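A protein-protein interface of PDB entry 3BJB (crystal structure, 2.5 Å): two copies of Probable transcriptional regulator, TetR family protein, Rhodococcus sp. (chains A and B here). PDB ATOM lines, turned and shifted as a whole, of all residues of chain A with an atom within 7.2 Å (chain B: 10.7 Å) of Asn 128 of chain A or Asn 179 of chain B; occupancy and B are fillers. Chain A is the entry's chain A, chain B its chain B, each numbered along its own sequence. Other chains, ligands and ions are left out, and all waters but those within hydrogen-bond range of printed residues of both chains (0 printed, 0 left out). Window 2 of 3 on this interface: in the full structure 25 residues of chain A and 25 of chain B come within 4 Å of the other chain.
OG1 of Thr 126 of chain A is in hydrogen-bond range of NE2 of Gln 122 of chain B (3.3 Å).
N of Val 129 of chain A lies within hydrogen-bond range of O of Asn 179 of chain B (2.8 Å).
O of Ser 125 of chain A lies within hydrogen-bond range of ND2 of Asn 179 of chain B (3.0 Å).
The side-chain amide nitrogen (ND2) of Asn 128 of chain A is in hydrogen-bond range of the backbone carbonyl oxygen (O) of Asn 179 of chain B, at 3.4 Å.
The side-chain hydroxyl (OG) of Ser 125 of chain A is in hydrogen-bond range of the side-chain amide nitrogen (NE2) of Gln 175 of chain B, at 3.4 Å.
The backbone carbonyl oxygen of Gln 175 of chain B is in hydrogen-bond range of the side-chain amide nitrogen of Asn 179 of chain B.
OD1 of Asn 128 of chain A sits at hydrogen-bond distance from N of Ala 130 of chain A (2.7 Å).
The backbone carbonyl oxygen of Ser 176 of chain B is in hydrogen-bond range of the backbone NH of Arg 181 of chain B (3.1 Å).
The backbone NH of Ser 131 of chain A is in hydrogen-bond range of the side-chain amide oxygen of Asn 128 of chain A (3.1 Å).
The side-chain hydroxyl (OG) of Ser 125 of chain B is in hydrogen-bond range of the side-chain amide nitrogen (NE2) of Gln 175 of chain B.
OD1 of Asn 179 of chain B touches O of Thr 126 of chain A (3.5 Å).
Asn 179 of chain B touches Ala 127 of chain A (CG to O, 3.2 Å).
Arg 181 of chain B touches Val 129 of chain A.
Arg 181 of chain B touches Ala 135 of chain A (CD to O, 3.5 Å).
Asn 128 of chain A touches just one residue of chain B: Asn 179 (3.4 Å).
Of chain A, only Ser 125 (3.0 Å), Thr 126 (3.5 Å), Ala 127 (3.2 Å), Asn 128 (3.4 Å) and Val 129 (2.8 Å) come within 4 Å of Asn 179 of chain B.
Of chain B, only Gln 175 and Asn 179 come within 4 Å of Ser 125 of chain A.
Of chain B, only Gln 122 (3.3 Å) and Asn 179 (3.5 Å) come within 4 Å of Thr 126 of chain A.
No residue of chain B comes within 4 Å of Ala 130 of chain A.
No residue of chain B comes within 4 Å of Ser 131 of chain A.
Printed residues of chain A within 4 Å of Gln 175 of chain B: Ser 125 (3.4 Å).
Printed residues of chain B within 4 Å of Ala 135 of chain A: Arg 181 (3.5 Å).
The nearest residue of chain B that does not touch Asn 128 of chain A is Leu 178 of chain B (4.3 Å).
The nearest residue of chain A that does not touch Asn 179 of chain B is Thr 124 of chain A (4.1 Å).
The nearest printed residue of chain B that does not touch Ala 135 of chain A is Asn 179 of chain B (6.6 Å).
Of the 16 printed residues of chain A, 6 touch a printed residue of chain B.
Along chain B the printed residues that touch a printed residue of chain A span positions 122 to 181.
Among the printed residues, 9 pairs touch across the chains.
Among the printed residues, no Asp or Glu carboxylate lies within 4 Å of a Lys or Arg side-chain nitrogen of the other chain.
1 position is printed for both chains.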
ATOM      1  N   THR A  67      14.364 -13.945 -12.679  1.00  0.00           N
ATOM      2  CA  THR A  67      12.926 -14.020 -12.739  1.00  0.00           C
ATOM      3  C   THR A  67      12.344 -13.917 -11.336  1.00  0.00           C
ATOM      4  O   THR A  67      11.384 -13.192 -11.166  1.00  0.00           O
ATOM      5  CB  THR A  67      12.421 -15.303 -13.408  1.00  0.00           C
ATOM      6  OG1 THR A  67      12.936 -15.397 -14.735  1.00  0.00           O
ATOM      7  CG2 THR A  67      10.908 -15.279 -13.511  1.00  0.00           C
ATOM      8  N   HIS A  68      12.901 -14.628 -10.342  1.00  0.00           N
ATOM      9  CA  HIS A  68      12.276 -14.658  -9.000  1.00  0.00           C
ATOM     10  C   HIS A  68      12.262 -13.299  -8.393  1.00  0.00           C
ATOM     11  O   HIS A  68      11.483 -13.034  -7.441  1.00  0.00           O
ATOM     12  CB  HIS A  68      13.032 -15.559  -8.020  1.00  0.00           C
ATOM     13  CG  HIS A  68      12.820 -17.022  -8.244  1.00  0.00           C
ATOM     14  ND1 HIS A  68      13.348 -17.696  -9.341  1.00  0.00           N
ATOM     15  CD2 HIS A  68      12.162 -17.947  -7.510  1.00  0.00           C
ATOM     16  CE1 HIS A  68      12.981 -18.965  -9.283  1.00  0.00           C
ATOM     17  NE2 HIS A  68      12.271 -19.143  -8.178  1.00  0.00           N
ATOM     18  N   SER A 123       9.127 -10.646 -16.702  1.00  0.00           N
ATOM     19  CA  SER A 123       9.343 -11.673 -15.687  1.00  0.00           C
ATOM     20  C   SER A 123       8.059 -12.283 -15.189  1.00  0.00           C
ATOM     21  O   SER A 123       7.972 -13.499 -15.045  1.00  0.00           O
ATOM     22  CB  SER A 123      10.083 -11.108 -14.496  1.00  0.00           C
ATOM     23  OG  SER A 123      11.397 -10.756 -14.866  1.00  0.00           O
ATOM     24  N   THR A 124       7.064 -11.448 -14.933  1.00  0.00           N
ATOM     25  CA  THR A 124       5.785 -11.976 -14.534  1.00  0.00           C
ATOM     26  C   THR A 124       5.110 -12.800 -15.647  1.00  0.00           C
ATOM     27  O   THR A 124       4.832 -13.978 -15.460  1.00  0.00           O
ATOM     28  CB  THR A 124       4.878 -10.898 -13.897  1.00  0.00           C
ATOM     29  OG1 THR A 124       5.623 -10.243 -12.859  1.00  0.00           O
ATOM     30  CG2 THR A 124       3.690 -11.546 -13.266  1.00  0.00           C
ATOM     31  N   SER A 125       4.906 -12.216 -16.822  1.00  0.00           N
ATOM     32  CA  SER A 125       4.128 -12.903 -17.826  1.00  0.00           C
ATOM     33  C   SER A 125       4.783 -14.223 -18.168  1.00  0.00           C
ATOM     34  O   SER A 125       4.163 -15.113 -18.752  1.00  0.00           O
ATOM     35  CB  SER A 125       3.950 -12.045 -19.071  1.00  0.00           C
ATOM     36  OG  SER A 125       5.105 -12.151 -19.873  1.00  0.00           O
ATOM     37  N   THR A 126       6.038 -14.358 -17.767  1.00  0.00           N
ATOM     38  CA  THR A 126       6.847 -15.526 -18.127  1.00  0.00           C
ATOM     39  C   THR A 126       7.002 -16.590 -17.036  1.00  0.00           C
ATOM     40  O   THR A 126       7.372 -17.714 -17.358  1.00  0.00           O
ATOM     41  CB  THR A 126       8.269 -15.097 -18.641  1.00  0.00           C
ATOM     42  OG1 THR A 126       8.595 -15.916 -19.748  1.00  0.00           O
ATOM     43  CG2 THR A 126       9.405 -15.210 -17.547  1.00  0.00           C
ATOM     44  N   ALA A 127       6.749 -16.242 -15.766  1.00  0.00           N
ATOM     45  CA  ALA A 127       7.128 -17.111 -14.618  1.00  0.00           C
ATOM     46  C   ALA A 127       6.180 -18.296 -14.386  1.00  0.00           C
ATOM     47  O   ALA A 127       4.986 -18.132 -14.183  1.00  0.00           O
ATOM     48  CB  ALA A 127       7.229 -16.275 -13.356  1.00  0.00           C
ATOM     49  N   ASN A 128       6.694 -19.504 -14.375  1.00  0.00           N
ATOM     50  CA  ASN A 128       5.813 -20.613 -14.033  1.00  0.00           C
ATOM     51  C   ASN A 128       5.589 -20.606 -12.507  1.00  0.00           C
ATOM     52  O   ASN A 128       6.513 -20.397 -11.750  1.00  0.00           O
ATOM     53  CB  ASN A 128       6.383 -21.951 -14.583  1.00  0.00           C
ATOM     54  CG  ASN A 128       5.780 -23.180 -13.919  1.00  0.00           C
ATOM     55  OD1 ASN A 128       6.086 -23.524 -12.761  1.00  0.00           O
ATOM     56  ND2 ASN A 128       4.931 -23.849 -14.643  1.00  0.00           N
ATOM     57  N   VAL A 129       4.359 -20.807 -12.055  1.00  0.00           N
ATOM     58  CA  VAL A 129       4.106 -20.728 -10.612  1.00  0.00           C
ATOM     59  C   VAL A 129       4.822 -21.795  -9.806  1.00  0.00           C
ATOM     60  O   VAL A 129       5.140 -21.551  -8.658  1.00  0.00           O
ATOM     61  CB  VAL A 129       2.639 -20.757 -10.220  1.00  0.00           C
ATOM     62  CG1 VAL A 129       2.529 -20.965  -8.712  1.00  0.00           C
ATOM     63  CG2 VAL A 129       1.994 -19.493 -10.590  1.00  0.00           C
ATOM     64  N   ALA A 130       5.094 -22.967 -10.358  1.00  0.00           N
ATOM     65  CA  ALA A 130       5.890 -23.899  -9.553  1.00  0.00           C
ATOM     66  C   ALA A 130       7.368 -23.477  -9.369  1.00  0.00           C
ATOM     67  O   ALA A 130       7.925 -23.652  -8.270  1.00  0.00           O
ATOM     68  CB  ALA A 130       5.769 -25.300 -10.068  1.00  0.00           C
ATOM     69  N   SER A 131       7.980 -22.908 -10.417  1.00  0.00           N
ATOM     70  CA  SER A 131       9.366 -22.410 -10.387  1.00  0.00           C
ATOM     71  C   SER A 131       9.498 -21.162  -9.581  1.00  0.00           C
ATOM     72  O   SER A 131      10.482 -20.982  -8.900  1.00  0.00           O
ATOM     73  CB  SER A 131       9.871 -22.017 -11.769  1.00  0.00           C
ATOM     74  OG  SER A 131      10.001 -23.120 -12.643  1.00  0.00           O
ATOM     75  N   VAL A 132       8.555 -20.238  -9.754  1.00  0.00           N
ATOM     76  CA  VAL A 132       8.597 -18.966  -9.022  1.00  0.00           C
ATOM     77  C   VAL A 132       7.301 -18.721  -8.251  1.00  0.00           C
ATOM     78  O   VAL A 132       6.290 -18.188  -8.778  1.00  0.00           O
ATOM     79  CB  VAL A 132       9.224 -17.774  -9.871  1.00  0.00           C
ATOM     80  CG1 VAL A 132       9.659 -18.225 -11.259  1.00  0.00           C
ATOM     81  CG2 VAL A 132       8.369 -16.521  -9.906  1.00  0.00           C
ATOM     82  N   PRO A 133       7.296 -19.203  -6.988  1.00  0.00           N
ATOM     83  CA  PRO A 133       6.090 -19.131  -6.168  1.00  0.00           C
ATOM     84  C   PRO A 133       5.516 -17.731  -6.102  1.00  0.00           C
ATOM     85  O   PRO A 133       4.309 -17.577  -6.106  1.00  0.00           O
ATOM     86  CB  PRO A 133       6.578 -19.579  -4.795  1.00  0.00           C
ATOM     87  CG  PRO A 133       7.753 -20.430  -5.066  1.00  0.00           C
ATOM     88  CD  PRO A 133       8.408 -19.863  -6.286  1.00  0.00           C
ATOM     89  N   ASP A 134       6.355 -16.701  -6.071  1.00  0.00           N
ATOM     90  CA  ASP A 134       5.803 -15.343  -5.899  1.00  0.00           C
ATOM     91  C   ASP A 134       4.861 -14.972  -7.033  1.00  0.00           C
ATOM     92  O   ASP A 134       4.084 -14.023  -6.913  1.00  0.00           O
ATOM     93  CB  ASP A 134       6.889 -14.270  -5.771  1.00  0.00           C
ATOM     94  CG  ASP A 134       7.503 -14.225  -4.416  1.00  0.00           C
ATOM     95  OD1 ASP A 134       7.044 -14.934  -3.501  1.00  0.00           O
ATOM     96  OD2 ASP A 134       8.487 -13.484  -4.246  1.00  0.00           O
ATOM     97  N   ALA A 135       4.943 -15.720  -8.119  1.00  0.00           N
ATOM     98  CA  ALA A 135       4.168 -15.423  -9.301  1.00  0.00           C
ATOM     99  C   ALA A 135       2.728 -15.755  -9.009  1.00  0.00           C
ATOM    100  O   ALA A 135       1.843 -15.127  -9.556  1.00  0.00           O
ATOM    101  CB  ALA A 135       4.668 -16.221 -10.514  1.00  0.00           C
ATOM    102  N   GLY A 136       2.491 -16.758  -8.169  1.00  0.00           N
ATOM    103  CA  GLY A 136       1.124 -17.094  -7.756  1.00  0.00           C
ATOM    104  C   GLY A 136       0.563 -16.169  -6.685  1.00  0.00           C
ATOM    105  O   GLY A 136      -0.452 -16.473  -6.073  1.00  0.00           O
ATOM    106  N   GLU B  39      11.969 -25.670 -24.831  1.00  0.00           N
ATOM    107  CA  GLU B  39      11.677 -24.251 -24.620  1.00  0.00           C
ATOM    108  C   GLU B  39      12.362 -23.292 -25.651  1.00  0.00           C
ATOM    109  O   GLU B  39      13.319 -23.682 -26.372  1.00  0.00           O
ATOM    110  CB  GLU B  39      12.110 -23.898 -23.207  1.00  0.00           C
ATOM    111  CG  GLU B  39      13.580 -24.228 -23.030  1.00  0.00           C
ATOM    112  CD  GLU B  39      14.085 -23.987 -21.631  1.00  0.00           C
ATOM    113  OE1 GLU B  39      13.908 -22.840 -21.113  1.00  0.00           O
ATOM    114  OE2 GLU B  39      14.675 -24.964 -21.069  1.00  0.00           O
ATOM    115  N   LEU B 110      -3.906 -24.741 -28.446  1.00  0.00           N
ATOM    116  CA  LEU B 110      -2.698 -24.178 -27.837  1.00  0.00           C
ATOM    117  C   LEU B 110      -2.245 -24.938 -26.603  1.00  0.00           C
ATOM    118  O   LEU B 110      -1.060 -25.285 -26.474  1.00  0.00           O
ATOM    119  CB  LEU B 110      -2.924 -22.721 -27.432  1.00  0.00           C
ATOM    120  CG  LEU B 110      -2.225 -21.548 -28.138  1.00  0.00           C
ATOM    121  CD1 LEU B 110      -2.190 -21.693 -29.641  1.00  0.00           C
ATOM    122  CD2 LEU B 110      -2.995 -20.300 -27.796  1.00  0.00           C
ATOM    123  N   LEU B 111      -3.176 -25.163 -25.675  1.00  0.00           N
ATOM    124  CA  LEU B 111      -2.896 -25.877 -24.434  1.00  0.00           C
ATOM    125  C   LEU B 111      -2.469 -27.317 -24.674  1.00  0.00           C
ATOM    126  O   LEU B 111      -1.878 -27.905 -23.793  1.00  0.00           O
ATOM    127  CB  LEU B 111      -4.096 -25.839 -23.535  1.00  0.00           C
ATOM    128  CG  LEU B 111      -4.279 -24.843 -22.383  1.00  0.00           C
ATOM    129  CD1 LEU B 111      -3.328 -23.636 -22.297  1.00  0.00           C
ATOM    130  CD2 LEU B 111      -5.682 -24.365 -22.485  1.00  0.00           C
ATOM    131  N   PRO B 114       2.032 -27.153 -25.038  1.00  0.00           N
ATOM    132  CA  PRO B 114       2.302 -26.005 -24.202  1.00  0.00           C
ATOM    133  C   PRO B 114       3.597 -25.418 -24.645  1.00  0.00           C
ATOM    134  O   PRO B 114       3.719 -24.186 -24.789  1.00  0.00           O
ATOM    135  CB  PRO B 114       2.441 -26.608 -22.789  1.00  0.00           C
ATOM    136  CG  PRO B 114       1.796 -27.975 -22.885  1.00  0.00           C
ATOM    137  CD  PRO B 114       2.112 -28.413 -24.270  1.00  0.00           C
ATOM    138  N   ALA B 115       4.562 -26.282 -24.909  1.00  0.00           N
ATOM    139  CA  ALA B 115       5.902 -25.808 -25.140  1.00  0.00           C
ATOM    140  C   ALA B 115       5.926 -24.902 -26.389  1.00  0.00           C
ATOM    141  O   ALA B 115       6.350 -23.749 -26.308  1.00  0.00           O
ATOM    142  CB  ALA B 115       6.894 -26.992 -25.208  1.00  0.00           C
ATOM    143  N   SER B 117       3.233 -23.446 -27.914  1.00  0.00           N
ATOM    144  CA  SER B 117       2.395 -22.288 -27.595  1.00  0.00           C
ATOM    145  C   SER B 117       3.087 -21.199 -26.788  1.00  0.00           C
ATOM    146  O   SER B 117       2.999 -20.014 -27.116  1.00  0.00           O
ATOM    147  CB  SER B 117       1.143 -22.768 -26.874  1.00  0.00           C
ATOM    148  OG  SER B 117       0.407 -23.569 -27.803  1.00  0.00           O
ATOM    149  N   THR B 118       3.804 -21.607 -25.752  1.00  0.00           N
ATOM    150  CA  THR B 118       4.617 -20.702 -25.002  1.00  0.00           C
ATOM    151  C   THR B 118       5.590 -19.963 -25.902  1.00  0.00           C
ATOM    152  O   THR B 118       5.696 -18.727 -25.810  1.00  0.00           O
ATOM    153  CB  THR B 118       5.363 -21.498 -23.969  1.00  0.00           C
ATOM    154  OG1 THR B 118       4.409 -22.227 -23.185  1.00  0.00           O
ATOM    155  CG2 THR B 118       6.203 -20.637 -23.112  1.00  0.00           C
ATOM    156  N   ALA B 119       6.296 -20.644 -26.798  1.00  0.00           N
ATOM    157  CA  ALA B 119       7.176 -19.894 -27.691  1.00  0.00           C
ATOM    158  C   ALA B 119       6.443 -18.902 -28.615  1.00  0.00           C
ATOM    159  O   ALA B 119       7.016 -17.871 -28.987  1.00  0.00           O
ATOM    160  CB  ALA B 119       8.030 -20.829 -28.507  1.00  0.00           C
ATOM    161  N   ILE B 121       3.348 -17.370 -28.040  1.00  0.00           N
ATOM    162  CA  ILE B 121       2.839 -16.360 -27.149  1.00  0.00           C
ATOM    163  C   ILE B 121       3.995 -15.439 -26.663  1.00  0.00           C
ATOM    164  O   ILE B 121       3.906 -14.203 -26.759  1.00  0.00           O
ATOM    165  CB  ILE B 121       2.133 -17.027 -25.941  1.00  0.00           C
ATOM    166  CG1 ILE B 121       1.043 -18.024 -26.394  1.00  0.00           C
ATOM    167  CG2 ILE B 121       1.650 -15.995 -24.903  1.00  0.00           C
ATOM    168  CD1 ILE B 121      -0.269 -17.424 -26.803  1.00  0.00           C
ATOM    169  N   GLN B 122       5.089 -16.005 -26.162  1.00  0.00           N
ATOM    170  CA  GLN B 122       6.120 -15.100 -25.660  1.00  0.00           C
ATOM    171  C   GLN B 122       6.641 -14.265 -26.761  1.00  0.00           C
ATOM    172  O   GLN B 122       6.839 -13.079 -26.571  1.00  0.00           O
ATOM    173  CB  GLN B 122       7.258 -15.789 -24.955  1.00  0.00           C
ATOM    174  CG  GLN B 122       6.855 -16.218 -23.605  1.00  0.00           C
ATOM    175  CD  GLN B 122       7.911 -17.094 -22.945  1.00  0.00           C
ATOM    176  OE1 GLN B 122       9.130 -16.964 -23.223  1.00  0.00           O
ATOM    177  NE2 GLN B 122       7.455 -17.991 -22.055  1.00  0.00           N
ATOM    178  N   SER B 125       4.288 -11.352 -27.446  1.00  0.00           N
ATOM    179  CA  SER B 125       4.391 -10.384 -26.365  1.00  0.00           C
ATOM    180  C   SER B 125       5.576  -9.451 -26.564  1.00  0.00           C
ATOM    181  O   SER B 125       5.396  -8.251 -26.564  1.00  0.00           O
ATOM    182  CB  SER B 125       4.495 -11.081 -25.019  1.00  0.00           C
ATOM    183  OG  SER B 125       3.292 -11.750 -24.747  1.00  0.00           O
ATOM    184  N   PHE B 171      -5.250 -13.558 -24.586  1.00  0.00           N
ATOM    185  CA  PHE B 171      -3.808 -13.801 -24.497  1.00  0.00           C
ATOM    186  C   PHE B 171      -3.344 -13.874 -23.058  1.00  0.00           C
ATOM    187  O   PHE B 171      -2.507 -14.694 -22.735  1.00  0.00           O
ATOM    188  CB  PHE B 171      -2.998 -12.717 -25.221  1.00  0.00           C
ATOM    189  CG  PHE B 171      -2.575 -13.112 -26.591  1.00  0.00           C
ATOM    190  CD1 PHE B 171      -1.238 -13.346 -26.875  1.00  0.00           C
ATOM    191  CD2 PHE B 171      -3.527 -13.268 -27.618  1.00  0.00           C
ATOM    192  CE1 PHE B 171      -0.848 -13.734 -28.171  1.00  0.00           C
ATOM    193  CE2 PHE B 171      -3.150 -13.647 -28.935  1.00  0.00           C
ATOM    194  CZ  PHE B 171      -1.813 -13.880 -29.207  1.00  0.00           C
ATOM    195  N   GLY B 172      -3.884 -13.012 -22.210  1.00  0.00           N
ATOM    196  CA  GLY B 172      -3.509 -13.022 -20.803  1.00  0.00           C
ATOM    197  C   GLY B 172      -3.905 -14.323 -20.124  1.00  0.00           C
ATOM    198  O   GLY B 172      -3.106 -14.911 -19.394  1.00  0.00           O
ATOM    199  N   VAL B 173      -5.130 -14.787 -20.406  1.00  0.00           N
ATOM    200  CA  VAL B 173      -5.661 -15.966 -19.763  1.00  0.00           C
ATOM    201  C   VAL B 173      -4.830 -17.181 -20.138  1.00  0.00           C
ATOM    202  O   VAL B 173      -4.526 -18.034 -19.259  1.00  0.00           O
ATOM    203  CB  VAL B 173      -7.132 -16.201 -20.147  1.00  0.00           C
ATOM    204  CG1 VAL B 173      -7.667 -17.415 -19.432  1.00  0.00           C
ATOM    205  CG2 VAL B 173      -7.998 -14.910 -19.874  1.00  0.00           C
ATOM    206  N   ILE B 174      -4.464 -17.277 -21.424  1.00  0.00           N
ATOM    207  CA  ILE B 174      -3.650 -18.405 -21.879  1.00  0.00           C
ATOM    208  C   ILE B 174      -2.285 -18.383 -21.201  1.00  0.00           C
ATOM    209  O   ILE B 174      -1.842 -19.391 -20.662  1.00  0.00           O
ATOM    210  CB  ILE B 174      -3.425 -18.420 -23.403  1.00  0.00           C
ATOM    211  CG1 ILE B 174      -4.730 -18.217 -24.127  1.00  0.00           C
ATOM    212  CG2 ILE B 174      -2.922 -19.791 -23.825  1.00  0.00           C
ATOM    213  CD1 ILE B 174      -5.626 -19.406 -23.995  1.00  0.00           C
ATOM    214  N   GLN B 175      -1.640 -17.226 -21.221  1.00  0.00           N
ATOM    215  CA  GLN B 175      -0.310 -17.070 -20.693  1.00  0.00           C
ATOM    216  C   GLN B 175      -0.350 -17.575 -19.254  1.00  0.00           C
ATOM    217  O   GLN B 175       0.494 -18.362 -18.804  1.00  0.00           O
ATOM    218  CB  GLN B 175       0.052 -15.581 -20.723  1.00  0.00           C
ATOM    219  CG  GLN B 175       1.488 -15.237 -21.168  1.00  0.00           C
ATOM    220  CD  GLN B 175       1.621 -13.754 -21.649  1.00  0.00           C
ATOM    221  OE1 GLN B 175       0.657 -12.988 -21.595  1.00  0.00           O
ATOM    222  NE2 GLN B 175       2.831 -13.367 -22.108  1.00  0.00           N
ATOM    223  N   SER B 176      -1.390 -17.121 -18.569  1.00  0.00           N
ATOM    224  CA  SER B 176      -1.669 -17.466 -17.202  1.00  0.00           C
ATOM    225  C   SER B 176      -1.857 -18.971 -16.958  1.00  0.00           C
ATOM    226  O   SER B 176      -1.318 -19.541 -15.998  1.00  0.00           O
ATOM    227  CB  SER B 176      -2.873 -16.671 -16.763  1.00  0.00           C
ATOM    228  OG  SER B 176      -3.337 -17.168 -15.556  1.00  0.00           O
ATOM    229  N   CYS B 177      -2.625 -19.578 -17.852  1.00  0.00           N
ATOM    230  CA  CYS B 177      -2.818 -21.010 -17.947  1.00  0.00           C
ATOM    231  C   CYS B 177      -1.538 -21.815 -18.188  1.00  0.00           C
ATOM    232  O   CYS B 177      -1.276 -22.794 -17.509  1.00  0.00           O
ATOM    233  CB  CYS B 177      -3.804 -21.282 -19.079  1.00  0.00           C
ATOM    234  SG  CYS B 177      -4.765 -22.781 -18.834  1.00  0.00           S
ATOM    235  N   LEU B 178      -0.736 -21.405 -19.162  1.00  0.00           N
ATOM    236  CA  LEU B 178       0.547 -22.034 -19.379  1.00  0.00           C
ATOM    237  C   LEU B 178       1.427 -21.965 -18.129  1.00  0.00           C
ATOM    238  O   LEU B 178       2.087 -22.922 -17.767  1.00  0.00           O
ATOM    239  CB  LEU B 178       1.211 -21.370 -20.553  1.00  0.00           C
ATOM    240  CG  LEU B 178       1.151 -21.972 -21.974  1.00  0.00           C
ATOM    241  CD1 LEU B 178       0.332 -23.251 -22.121  1.00  0.00           C
ATOM    242  CD2 LEU B 178       0.748 -20.881 -22.981  1.00  0.00           C
ATOM    243  N   ASN B 179       1.380 -20.852 -17.409  1.00  0.00           N
ATOM    244  CA  ASN B 179       2.179 -20.708 -16.195  1.00  0.00           C
ATOM    245  C   ASN B 179       1.674 -21.416 -14.962  1.00  0.00           C
ATOM    246  O   ASN B 179       2.428 -21.580 -13.998  1.00  0.00           O
ATOM    247  CB  ASN B 179       2.339 -19.260 -15.857  1.00  0.00           C
ATOM    248  CG  ASN B 179       3.198 -18.538 -16.836  1.00  0.00           C
ATOM    249  OD1 ASN B 179       4.155 -19.124 -17.436  1.00  0.00           O
ATOM    250  ND2 ASN B 179       2.907 -17.236 -16.997  1.00  0.00           N
ATOM    251  N   GLY B 180       0.409 -21.819 -14.983  1.00  0.00           N
ATOM    252  CA  GLY B 180      -0.141 -22.736 -13.985  1.00  0.00           C
ATOM    253  C   GLY B 180      -0.869 -21.990 -12.883  1.00  0.00           C
ATOM    254  O   GLY B 180      -1.087 -22.558 -11.799  1.00  0.00           O
ATOM    255  N   ARG B 181      -1.232 -20.741 -13.194  1.00  0.00           N
ATOM    256  CA  ARG B 181      -1.956 -19.818 -12.337  1.00  0.00           C
ATOM    257  C   ARG B 181      -3.446 -20.046 -12.355  1.00  0.00           C
ATOM    258  O   ARG B 181      -4.103 -19.814 -11.361  1.00  0.00           O
ATOM    259  CB  ARG B 181      -1.688 -18.350 -12.730  1.00  0.00           C
ATOM    260  CG  ARG B 181      -0.288 -17.810 -12.257  1.00  0.00           C
ATOM    261  CD  ARG B 181      -0.209 -16.283 -12.168  1.00  0.00           C
ATOM    262  NE  ARG B 181      -1.068 -15.751 -13.203  1.00  0.00           N
ATOM    263  CZ  ARG B 181      -0.985 -14.553 -13.777  1.00  0.00           C
ATOM    264  NH1 ARG B 181      -1.876 -14.245 -14.747  1.00  0.00           N
ATOM    265  NH2 ARG B 181      -0.044 -13.680 -13.412  1.00  0.00           N
ATOM    266  N   VAL B 182      -3.995 -20.447 -13.493  1.00  0.00           N
ATOM    267  CA  VAL B 182      -5.401 -20.807 -13.556  1.00  0.00           C
ATOM    268  C   VAL B 182      -5.491 -22.244 -14.080  1.00  0.00           C
ATOM    269  O   VAL B 182      -4.606 -22.690 -14.819  1.00  0.00           O
ATOM    270  CB  VAL B 182      -6.186 -19.802 -14.416  1.00  0.00           C
ATOM    271  CG1 VAL B 182      -5.920 -20.005 -15.918  1.00  0.00           C
ATOM    272  CG2 VAL B 182      -7.686 -19.879 -14.127  1.00  0.00           C
ATOM    273  N   SER B 183      -6.493 -23.001 -13.655  1.00  0.00           N
ATOM    274  CA  SER B 183      -6.729 -24.321 -14.244  1.00  0.00           C
ATOM    275  C   SER B 183      -7.386 -24.142 -15.610  1.00  0.00           C
ATOM    276  O   SER B 183      -7.754 -23.024 -15.984  1.00  0.00           O
ATOM    277  CB  SER B 183      -7.618 -25.171 -13.367  1.00  0.00           C
ATOM    278  OG  SER B 183      -8.924 -24.685 -13.456  1.00  0.00           O
ATOM    279  N   ILE B 184      -7.545 -25.224 -16.374  1.00  0.00           N
ATOM    280  CA  ILE B 184      -8.042 -24.992 -17.715  1.00  0.00           C
ATOM    281  C   ILE B 184      -9.556 -24.753 -17.776  1.00  0.00           C
ATOM    282  O   ILE B 184     -10.011 -23.872 -18.510  1.00  0.00           O
ATOM    283  CB  ILE B 184      -7.422 -25.884 -18.877  1.00  0.00           C
ATOM    284  CG1 ILE B 184      -8.473 -26.663 -19.604  1.00  0.00           C
ATOM    285  CG2 ILE B 184      -6.170 -26.696 -18.544  1.00  0.00           C
ATOM    286  CD1 ILE B 184      -8.637 -26.081 -20.917  1.00  0.00           C
ATOM    287  N   ALA B 187      -9.928 -21.288 -16.927  1.00  0.00           N
ATOM    288  CA  ALA B 187      -9.545 -20.423 -18.057  1.00  0.00           C
ATOM    289  C   ALA B 187     -10.723 -20.294 -18.995  1.00  0.00           C
ATOM    290  O   ALA B 187     -11.182 -19.167 -19.300  1.00  0.00           O
ATOM    291  CB  ALA B 187      -8.350 -20.970 -18.813  1.00  0.00           C
